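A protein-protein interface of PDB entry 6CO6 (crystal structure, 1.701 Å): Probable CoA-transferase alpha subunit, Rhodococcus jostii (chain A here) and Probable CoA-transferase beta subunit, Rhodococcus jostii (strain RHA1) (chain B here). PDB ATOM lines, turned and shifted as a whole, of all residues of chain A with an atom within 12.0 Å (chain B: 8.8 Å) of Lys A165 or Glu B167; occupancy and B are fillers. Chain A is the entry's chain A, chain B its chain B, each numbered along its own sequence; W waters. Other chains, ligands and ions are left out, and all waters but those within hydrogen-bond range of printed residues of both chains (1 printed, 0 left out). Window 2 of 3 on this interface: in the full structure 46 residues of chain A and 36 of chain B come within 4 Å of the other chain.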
ATOM      1  N   LEU A 140     -24.095 -26.414  -6.594  1.00  0.00           N
ATOM      2  CA  LEU A 140     -22.980 -26.140  -5.689  1.00  0.00           C
ATOM      3  C   LEU A 140     -22.039 -27.331  -5.593  1.00  0.00           C
ATOM      4  O   LEU A 140     -22.473 -28.478  -5.470  1.00  0.00           O
ATOM      5  CB  LEU A 140     -23.501 -25.811  -4.289  1.00  0.00           C
ATOM      6  CG  LEU A 140     -24.116 -24.448  -4.040  1.00  0.00           C
ATOM      7  CD1 LEU A 140     -24.672 -24.439  -2.611  1.00  0.00           C
ATOM      8  CD2 LEU A 140     -23.071 -23.358  -4.227  1.00  0.00           C
ATOM      9  N   VAL A 155     -25.819 -16.363  -4.983  1.00  0.00           N
ATOM     10  CA  VAL A 155     -26.516 -15.315  -4.253  1.00  0.00           C
ATOM     11  C   VAL A 155     -26.477 -15.677  -2.775  1.00  0.00           C
ATOM     12  O   VAL A 155     -26.658 -16.841  -2.400  1.00  0.00           O
ATOM     13  CB  VAL A 155     -27.962 -15.128  -4.766  1.00  0.00           C
ATOM     14  CG1 VAL A 155     -28.770 -16.422  -4.639  1.00  0.00           C
ATOM     15  CG2 VAL A 155     -28.648 -13.977  -4.030  1.00  0.00           C
ATOM     16  N   THR A 156     -26.210 -14.694  -1.931  1.00  0.00           N
ATOM     17  CA  THR A 156     -26.155 -14.935  -0.495  1.00  0.00           C
ATOM     18  C   THR A 156     -27.452 -14.489   0.161  1.00  0.00           C
ATOM     19  O   THR A 156     -27.970 -13.408  -0.141  1.00  0.00           O
ATOM     20  CB  THR A 156     -24.969 -14.216   0.135  1.00  0.00           C
ATOM     21  OG1 THR A 156     -23.763 -14.698  -0.460  1.00  0.00           O
ATOM     22  CG2 THR A 156     -24.923 -14.491   1.648  1.00  0.00           C
ATOM     23  N   SER A 157     -27.974 -15.330   1.042  1.00  0.00           N
ATOM     24  CA  SER A 157     -29.180 -14.996   1.783  1.00  0.00           C
ATOM     25  C   SER A 157     -28.969 -13.725   2.600  1.00  0.00           C
ATOM     26  O   SER A 157     -27.948 -13.600   3.289  1.00  0.00           O
ATOM     27  CB  SER A 157     -29.546 -16.145   2.719  1.00  0.00           C
ATOM     28  OG  SER A 157     -30.663 -15.814   3.521  1.00  0.00           O
ATOM     29  N   PRO A 158     -29.905 -12.771   2.574  1.00  0.00           N
ATOM     30  CA  PRO A 158     -29.825 -11.641   3.513  1.00  0.00           C
ATOM     31  C   PRO A 158     -30.214 -12.007   4.938  1.00  0.00           C
ATOM     32  O   PRO A 158     -30.109 -11.150   5.830  1.00  0.00           O
ATOM     33  CB  PRO A 158     -30.813 -10.626   2.921  1.00  0.00           C
ATOM     34  CG  PRO A 158     -31.816 -11.467   2.229  1.00  0.00           C
ATOM     35  CD  PRO A 158     -31.047 -12.642   1.651  1.00  0.00           C
ATOM     36  N   TYR A 159     -30.655 -13.245   5.170  1.00  0.00           N
ATOM     37  CA  TYR A 159     -30.971 -13.762   6.497  1.00  0.00           C
ATOM     38  C   TYR A 159     -29.977 -14.851   6.856  1.00  0.00           C
ATOM     39  O   TYR A 159     -29.927 -15.867   6.146  1.00  0.00           O
ATOM     40  CB  TYR A 159     -32.387 -14.331   6.541  1.00  0.00           C
ATOM     41  CG  TYR A 159     -33.435 -13.448   5.935  1.00  0.00           C
ATOM     42  CD1 TYR A 159     -33.847 -12.294   6.584  1.00  0.00           C
ATOM     43  CD2 TYR A 159     -34.023 -13.771   4.723  1.00  0.00           C
ATOM     44  CE1 TYR A 159     -34.813 -11.474   6.038  1.00  0.00           C
ATOM     45  CE2 TYR A 159     -34.989 -12.961   4.170  1.00  0.00           C
ATOM     46  CZ  TYR A 159     -35.372 -11.810   4.826  1.00  0.00           C
ATOM     47  OH  TYR A 159     -36.338 -11.000   4.278  1.00  0.00           O
ATOM     48  N   PRO A 160     -29.175 -14.715   7.910  1.00  0.00           N
ATOM     49  CA  PRO A 160     -28.328 -15.837   8.317  1.00  0.00           C
ATOM     50  C   PRO A 160     -29.177 -16.976   8.863  1.00  0.00           C
ATOM     51  O   PRO A 160     -30.337 -16.800   9.257  1.00  0.00           O
ATOM     52  CB  PRO A 160     -27.420 -15.239   9.404  1.00  0.00           C
ATOM     53  CG  PRO A 160     -27.504 -13.738   9.199  1.00  0.00           C
ATOM     54  CD  PRO A 160     -28.914 -13.509   8.715  1.00  0.00           C
ATOM     55  N   ASP A 161     -28.583 -18.166   8.871  1.00  0.00           N
ATOM     56  CA  ASP A 161     -29.226 -19.306   9.509  1.00  0.00           C
ATOM     57  C   ASP A 161     -29.122 -19.163  11.033  1.00  0.00           C
ATOM     58  O   ASP A 161     -28.503 -18.234  11.563  1.00  0.00           O
ATOM     59  CB  ASP A 161     -28.601 -20.619   9.023  1.00  0.00           C
ATOM     60  CG  ASP A 161     -29.007 -21.009   7.571  1.00  0.00           C
ATOM     61  OD1 ASP A 161     -29.682 -20.247   6.832  1.00  0.00           O
ATOM     62  OD2 ASP A 161     -28.633 -22.128   7.158  1.00  0.00           O
ATOM     63  N   ALA A 162     -29.731 -20.110  11.756  1.00  0.00           N
ATOM     64  CA  ALA A 162     -29.738 -20.037  13.215  1.00  0.00           C
ATOM     65  C   ALA A 162     -28.331 -20.057  13.797  1.00  0.00           C
ATOM     66  O   ALA A 162     -28.111 -19.554  14.901  1.00  0.00           O
ATOM     67  CB  ALA A 162     -30.567 -21.185  13.795  1.00  0.00           C
ATOM     68  N   SER A 163     -27.366 -20.633  13.076  1.00  0.00           N
ATOM     69  CA  SER A 163     -25.991 -20.663  13.559  1.00  0.00           C
ATOM     70  C   SER A 163     -25.297 -19.310  13.469  1.00  0.00           C
ATOM     71  O   SER A 163     -24.203 -19.156  14.028  1.00  0.00           O
ATOM     72  CB  SER A 163     -25.195 -21.690  12.755  1.00  0.00           C
ATOM     73  OG  SER A 163     -25.213 -21.345  11.379  1.00  0.00           O
ATOM     74  N   GLY A 164     -25.890 -18.336  12.779  1.00  0.00           N
ATOM     75  CA  GLY A 164     -25.223 -17.091  12.481  1.00  0.00           C
ATOM     76  C   GLY A 164     -24.561 -17.043  11.116  1.00  0.00           C
ATOM     77  O   GLY A 164     -24.043 -15.989  10.736  1.00  0.00           O
ATOM     78  N   LYS A 165     -24.558 -18.142  10.377  1.00  0.00           N
ATOM     79  CA  LYS A 165     -23.918 -18.185   9.065  1.00  0.00           C
ATOM     80  C   LYS A 165     -24.959 -17.991   7.971  1.00  0.00           C
ATOM     81  O   LYS A 165     -26.044 -18.574   8.026  1.00  0.00           O
ATOM     82  CB  LYS A 165     -23.196 -19.512   8.833  1.00  0.00           C
ATOM     83  CG  LYS A 165     -22.037 -19.796   9.759  1.00  0.00           C
ATOM     84  CD  LYS A 165     -21.434 -21.149   9.388  1.00  0.00           C
ATOM     85  CE  LYS A 165     -20.311 -21.545  10.294  1.00  0.00           C
ATOM     86  NZ  LYS A 165     -20.765 -21.718  11.702  1.00  0.00           N
ATOM     87  N   SER A 166     -24.597 -17.214   6.948  1.00  0.00           N
ATOM     88  CA  SER A 166     -25.480 -16.968   5.811  1.00  0.00           C
ATOM     89  C   SER A 166     -25.216 -17.983   4.708  1.00  0.00           C
ATOM     90  O   SER A 166     -24.060 -18.219   4.330  1.00  0.00           O
ATOM     91  CB  SER A 166     -25.278 -15.556   5.263  1.00  0.00           C
ATOM     92  OG  SER A 166     -25.440 -14.588   6.282  1.00  0.00           O
ATOM     93  N   GLU A 167     -26.289 -18.552   4.167  1.00  0.00           N
ATOM     94  CA  GLU A 167     -26.156 -19.498   3.066  1.00  0.00           C
ATOM     95  C   GLU A 167     -25.871 -18.769   1.765  1.00  0.00           C
ATOM     96  O   GLU A 167     -26.498 -17.753   1.454  1.00  0.00           O
ATOM     97  CB  GLU A 167     -27.434 -20.315   2.908  1.00  0.00           C
ATOM     98  CG  GLU A 167     -27.698 -21.248   4.024  1.00  0.00           C
ATOM     99  CD  GLU A 167     -28.836 -22.178   3.700  1.00  0.00           C
ATOM    100  OE1 GLU A 167     -28.970 -22.551   2.528  1.00  0.00           O
ATOM    101  OE2 GLU A 167     -29.594 -22.542   4.607  1.00  0.00           O
ATOM    102  N   THR A 168     -24.939 -19.307   0.986  1.00  0.00           N
ATOM    103  CA  THR A 168     -24.695 -18.828  -0.362  1.00  0.00           C
ATOM    104  C   THR A 168     -25.089 -19.945  -1.319  1.00  0.00           C
ATOM    105  O   THR A 168     -24.597 -21.073  -1.204  1.00  0.00           O
ATOM    106  CB  THR A 168     -23.241 -18.398  -0.531  1.00  0.00           C
ATOM    107  OG1 THR A 168     -23.026 -17.229   0.273  1.00  0.00           O
ATOM    108  CG2 THR A 168     -22.946 -18.057  -1.984  1.00  0.00           C
ATOM    109  N   LEU A 169     -26.027 -19.639  -2.204  1.00  0.00           N
ATOM    110  CA  LEU A 169     -26.690 -20.616  -3.054  1.00  0.00           C
ATOM    111  C   LEU A 169     -26.446 -20.271  -4.513  1.00  0.00           C
ATOM    112  O   LEU A 169     -26.079 -19.143  -4.842  1.00  0.00           O
ATOM    113  CB  LEU A 169     -28.199 -20.628  -2.770  1.00  0.00           C
ATOM    114  CG  LEU A 169     -28.521 -21.013  -1.331  1.00  0.00           C
ATOM    115  CD1 LEU A 169     -29.768 -20.304  -0.806  1.00  0.00           C
ATOM    116  CD2 LEU A 169     -28.653 -22.517  -1.291  1.00  0.00           C
ATOM    117  N   ILE B 164     -16.723 -29.417  -0.097  1.00  0.00           N
ATOM    118  CA  ILE B 164     -17.597 -28.811   0.903  1.00  0.00           C
ATOM    119  C   ILE B 164     -16.951 -27.543   1.443  1.00  0.00           C
ATOM    120  O   ILE B 164     -15.765 -27.532   1.793  1.00  0.00           O
ATOM    121  CB  ILE B 164     -17.885 -29.808   2.035  1.00  0.00           C
ATOM    122  CG1 ILE B 164     -18.542 -31.089   1.498  1.00  0.00           C
ATOM    123  CG2 ILE B 164     -18.718 -29.145   3.148  1.00  0.00           C
ATOM    124  CD1 ILE B 164     -19.703 -30.858   0.559  1.00  0.00           C
ATOM    125  N   ASP B 165     -17.726 -26.455   1.499  1.00  0.00           N
ATOM    126  CA  ASP B 165     -17.284 -25.241   2.170  1.00  0.00           C
ATOM    127  C   ASP B 165     -17.873 -25.258   3.568  1.00  0.00           C
ATOM    128  O   ASP B 165     -19.096 -25.123   3.712  1.00  0.00           O
ATOM    129  CB  ASP B 165     -17.742 -23.993   1.408  1.00  0.00           C
ATOM    130  CG  ASP B 165     -17.308 -22.683   2.079  1.00  0.00           C
ATOM    131  OD1 ASP B 165     -16.660 -22.696   3.151  1.00  0.00           O
ATOM    132  OD2 ASP B 165     -17.619 -21.619   1.507  1.00  0.00           O
ATOM    133  N   PRO B 166     -17.064 -25.426   4.619  1.00  0.00           N
ATOM    134  CA  PRO B 166     -17.635 -25.541   5.969  1.00  0.00           C
ATOM    135  C   PRO B 166     -18.242 -24.248   6.481  1.00  0.00           C
ATOM    136  O   PRO B 166     -19.023 -24.285   7.440  1.00  0.00           O
ATOM    137  CB  PRO B 166     -16.430 -25.967   6.819  1.00  0.00           C
ATOM    138  CG  PRO B 166     -15.260 -25.377   6.104  1.00  0.00           C
ATOM    139  CD  PRO B 166     -15.592 -25.425   4.631  1.00  0.00           C
ATOM    140  N   GLU B 167     -17.915 -23.110   5.866  1.00  0.00           N
ATOM    141  CA  GLU B 167     -18.469 -21.823   6.269  1.00  0.00           C
ATOM    142  C   GLU B 167     -19.840 -21.550   5.670  1.00  0.00           C
ATOM    143  O   GLU B 167     -20.502 -20.591   6.090  1.00  0.00           O
ATOM    144  CB  GLU B 167     -17.520 -20.694   5.867  1.00  0.00           C
ATOM    145  CG  GLU B 167     -16.115 -20.826   6.420  1.00  0.00           C
ATOM    146  CD  GLU B 167     -15.190 -19.739   5.911  1.00  0.00           C
ATOM    147  OE1 GLU B 167     -15.607 -18.936   5.048  1.00  0.00           O
ATOM    148  OE2 GLU B 167     -14.037 -19.696   6.363  1.00  0.00           O
ATOM    149  N   ASN B 168     -20.267 -22.350   4.694  1.00  0.00           N
ATOM    150  CA  ASN B 168     -21.497 -22.096   3.962  1.00  0.00           C
ATOM    151  C   ASN B 168     -22.515 -23.182   4.275  1.00  0.00           C
ATOM    152  O   ASN B 168     -22.375 -24.316   3.789  1.00  0.00           O
ATOM    153  CB  ASN B 168     -21.208 -22.033   2.460  1.00  0.00           C
ATOM    154  CG  ASN B 168     -22.453 -21.784   1.629  1.00  0.00           C
ATOM    155  OD1 ASN B 168     -23.545 -21.563   2.158  1.00  0.00           O
ATOM    156  ND2 ASN B 168     -22.291 -21.803   0.315  1.00  0.00           N
ATOM    157  N   PRO B 169     -23.553 -22.881   5.063  1.00  0.00           N
ATOM    158  CA  PRO B 169     -24.517 -23.923   5.461  1.00  0.00           C
ATOM    159  C   PRO B 169     -25.293 -24.507   4.308  1.00  0.00           C
ATOM    160  O   PRO B 169     -26.002 -25.500   4.514  1.00  0.00           O
ATOM    161  CB  PRO B 169     -25.460 -23.194   6.433  1.00  0.00           C
ATOM    162  CG  PRO B 169     -24.737 -21.978   6.856  1.00  0.00           C
ATOM    163  CD  PRO B 169     -23.795 -21.598   5.742  1.00  0.00           C
ATOM    164  N   ALA B 170     -25.204 -23.930   3.107  1.00  0.00           N
ATOM    165  CA  ALA B 170     -25.849 -24.550   1.956  1.00  0.00           C
ATOM    166  C   ALA B 170     -25.331 -25.962   1.709  1.00  0.00           C
ATOM    167  O   ALA B 170     -26.003 -26.750   1.035  1.00  0.00           O
ATOM    168  CB  ALA B 170     -25.635 -23.688   0.707  1.00  0.00           C
ATOM    169  N   TYR B 171     -24.147 -26.288   2.230  1.00  0.00           N
ATOM    170  CA  TYR B 171     -23.516 -27.594   2.057  1.00  0.00           C
ATOM    171  C   TYR B 171     -23.839 -28.578   3.174  1.00  0.00           C
ATOM    172  O   TYR B 171     -23.284 -29.679   3.183  1.00  0.00           O
ATOM    173  CB  TYR B 171     -21.989 -27.442   1.989  1.00  0.00           C
ATOM    174  CG  TYR B 171     -21.431 -26.911   0.681  1.00  0.00           C
ATOM    175  CD1 TYR B 171     -21.141 -27.771  -0.372  1.00  0.00           C
ATOM    176  CD2 TYR B 171     -21.167 -25.550   0.517  1.00  0.00           C
ATOM    177  CE1 TYR B 171     -20.610 -27.292  -1.566  1.00  0.00           C
ATOM    178  CE2 TYR B 171     -20.636 -25.061  -0.669  1.00  0.00           C
ATOM    179  CZ  TYR B 171     -20.368 -25.939  -1.706  1.00  0.00           C
ATOM    180  OH  TYR B 171     -19.848 -25.462  -2.887  1.00  0.00           O
ATOM    181  N   ARG B 172     -24.698 -28.217   4.130  1.00  0.00           N
ATOM    182  CA  ARG B 172     -24.801 -29.019   5.342  1.00  0.00           C
ATOM    183  C   ARG B 172     -25.552 -30.332   5.166  1.00  0.00           C
ATOM    184  O   ARG B 172     -25.534 -31.150   6.090  1.00  0.00           O
ATOM    185  CB  ARG B 172     -25.478 -28.214   6.444  1.00  0.00           C
ATOM    186  CG  ARG B 172     -26.962 -27.974   6.226  1.00  0.00           C
ATOM    187  CD  ARG B 172     -27.443 -27.034   7.325  1.00  0.00           C
ATOM    188  NE  ARG B 172     -28.867 -26.747   7.279  1.00  0.00           N
ATOM    189  CZ  ARG B 172     -29.433 -25.878   6.450  1.00  0.00           C
ATOM    190  NH1 ARG B 172     -28.691 -25.228   5.566  1.00  0.00           N
ATOM    191  NH2 ARG B 172     -30.743 -25.661   6.509  1.00  0.00           N
HETATM  192  O   HOH W   1     -31.782 -23.658   4.713  1.00  0.00           O
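Leu A140 touches Ala B170. Leu A140 touches Tyr B171 (CB to OH, 3.9 Å). Pro B169 touches Asp A161. Glu B167 touches Lys A165 (O to CD, 3.5 Å). O of Ser A166 touches CD of Pro B169 (3.7 Å). Glu A167 touches Asn B168. Glu A167 touches Pro B169 (CG to CB, 3.8 Å). CA of Ala B170 touches OE1 of Glu A167, 3.8 Å away. Thr A168 touches Ala B170 (O to CB, 3.4 Å). Leu A169 touches Ala B170.
The side-chain carboxylate (OE2) of Glu A167 lies within salt-bridge range of the guanidinium group (NH1) of Arg B172 (3.0 Å). The side-chain amide nitrogen (ND2) of Asn B168 is in hydrogen-bond range of the backbone carbonyl oxygen (O) of Thr A168 (2.9 Å). OD2 of Asp A161 is in salt-bridge range of NH1 of Arg B172 (3.5 Å).
Of the 16 printed residues of chain A, 7 touch a printed residue of chain B. Hydrophobic or aromatic side chains of chain A that line the printed part of chain B: Leu A140 and Leu A169. Hydrophobic or aromatic side chains of chain B that line the printed part of chain A: Pro B169, Ala B170 and Tyr B171. Among the printed residues, Asp or Glu carboxylates within 4 Å of a Lys or Arg side-chain nitrogen of the other chain: Asp A161 with Arg B172 (3.5 Å) and Glu A167 with Arg B172 (3.0 Å).
Lys A165 touches two residues of chain B. Glu B167 touches one residue of chain A. No residue of chain B comes within 4 Å of Ser A163. No residue of chain B comes within 4 Å of Gly A164. Ser A166 touches just one residue of chain B: Pro B169 (3.7 Å). No residue of chain A comes within 4 Å of Asp B165. Asn B168 touches just these residues of chain A: Glu A167 (3.5 Å) and Thr A168 (2.9 Å). Printed residues of chain B within 4 Å of Thr A168: Asn B168 (2.9 Å) and Ala B170 (3.4 Å). Of the printed residues of chain B, Leu A140 touches Ala B170 and Tyr B171. Of the printed residues of chain A, Arg B172 touches Asp A161 and Glu A167. Of the printed residues of chain A, Tyr B171 touches Leu A140 (3.9 Å). The nearest residue of chain A that does not touch Glu B167 is Ser A166 (4.6 Å).
OD1 of Asp B165 lies within hydrogen-bond range of N of Glu B167, 3.0 Å away. O of Pro B169 sits at hydrogen-bond distance from NH1 of Arg B172, 2.9 Å away. The backbone carbonyl oxygen of Glu A167 sits at hydrogen-bond distance from the backbone NH of Ser A157, at 2.9 Å. N of Val A155 sits at hydrogen-bond distance from O of Leu A169 (2.8 Å). N of Ala B170 sits close to OD1 of Asn B168. The side-chain hydroxyl (OG1) of Thr A156 sits at hydrogen-bond distance from the side-chain hydroxyl (OG1) of Thr A168, 2.7 Å away.
Water W1 lies within hydrogen-bond range of OE2 of Glu A167 (2.5 Å) and NH2 of Arg B172 (2.9 Å).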
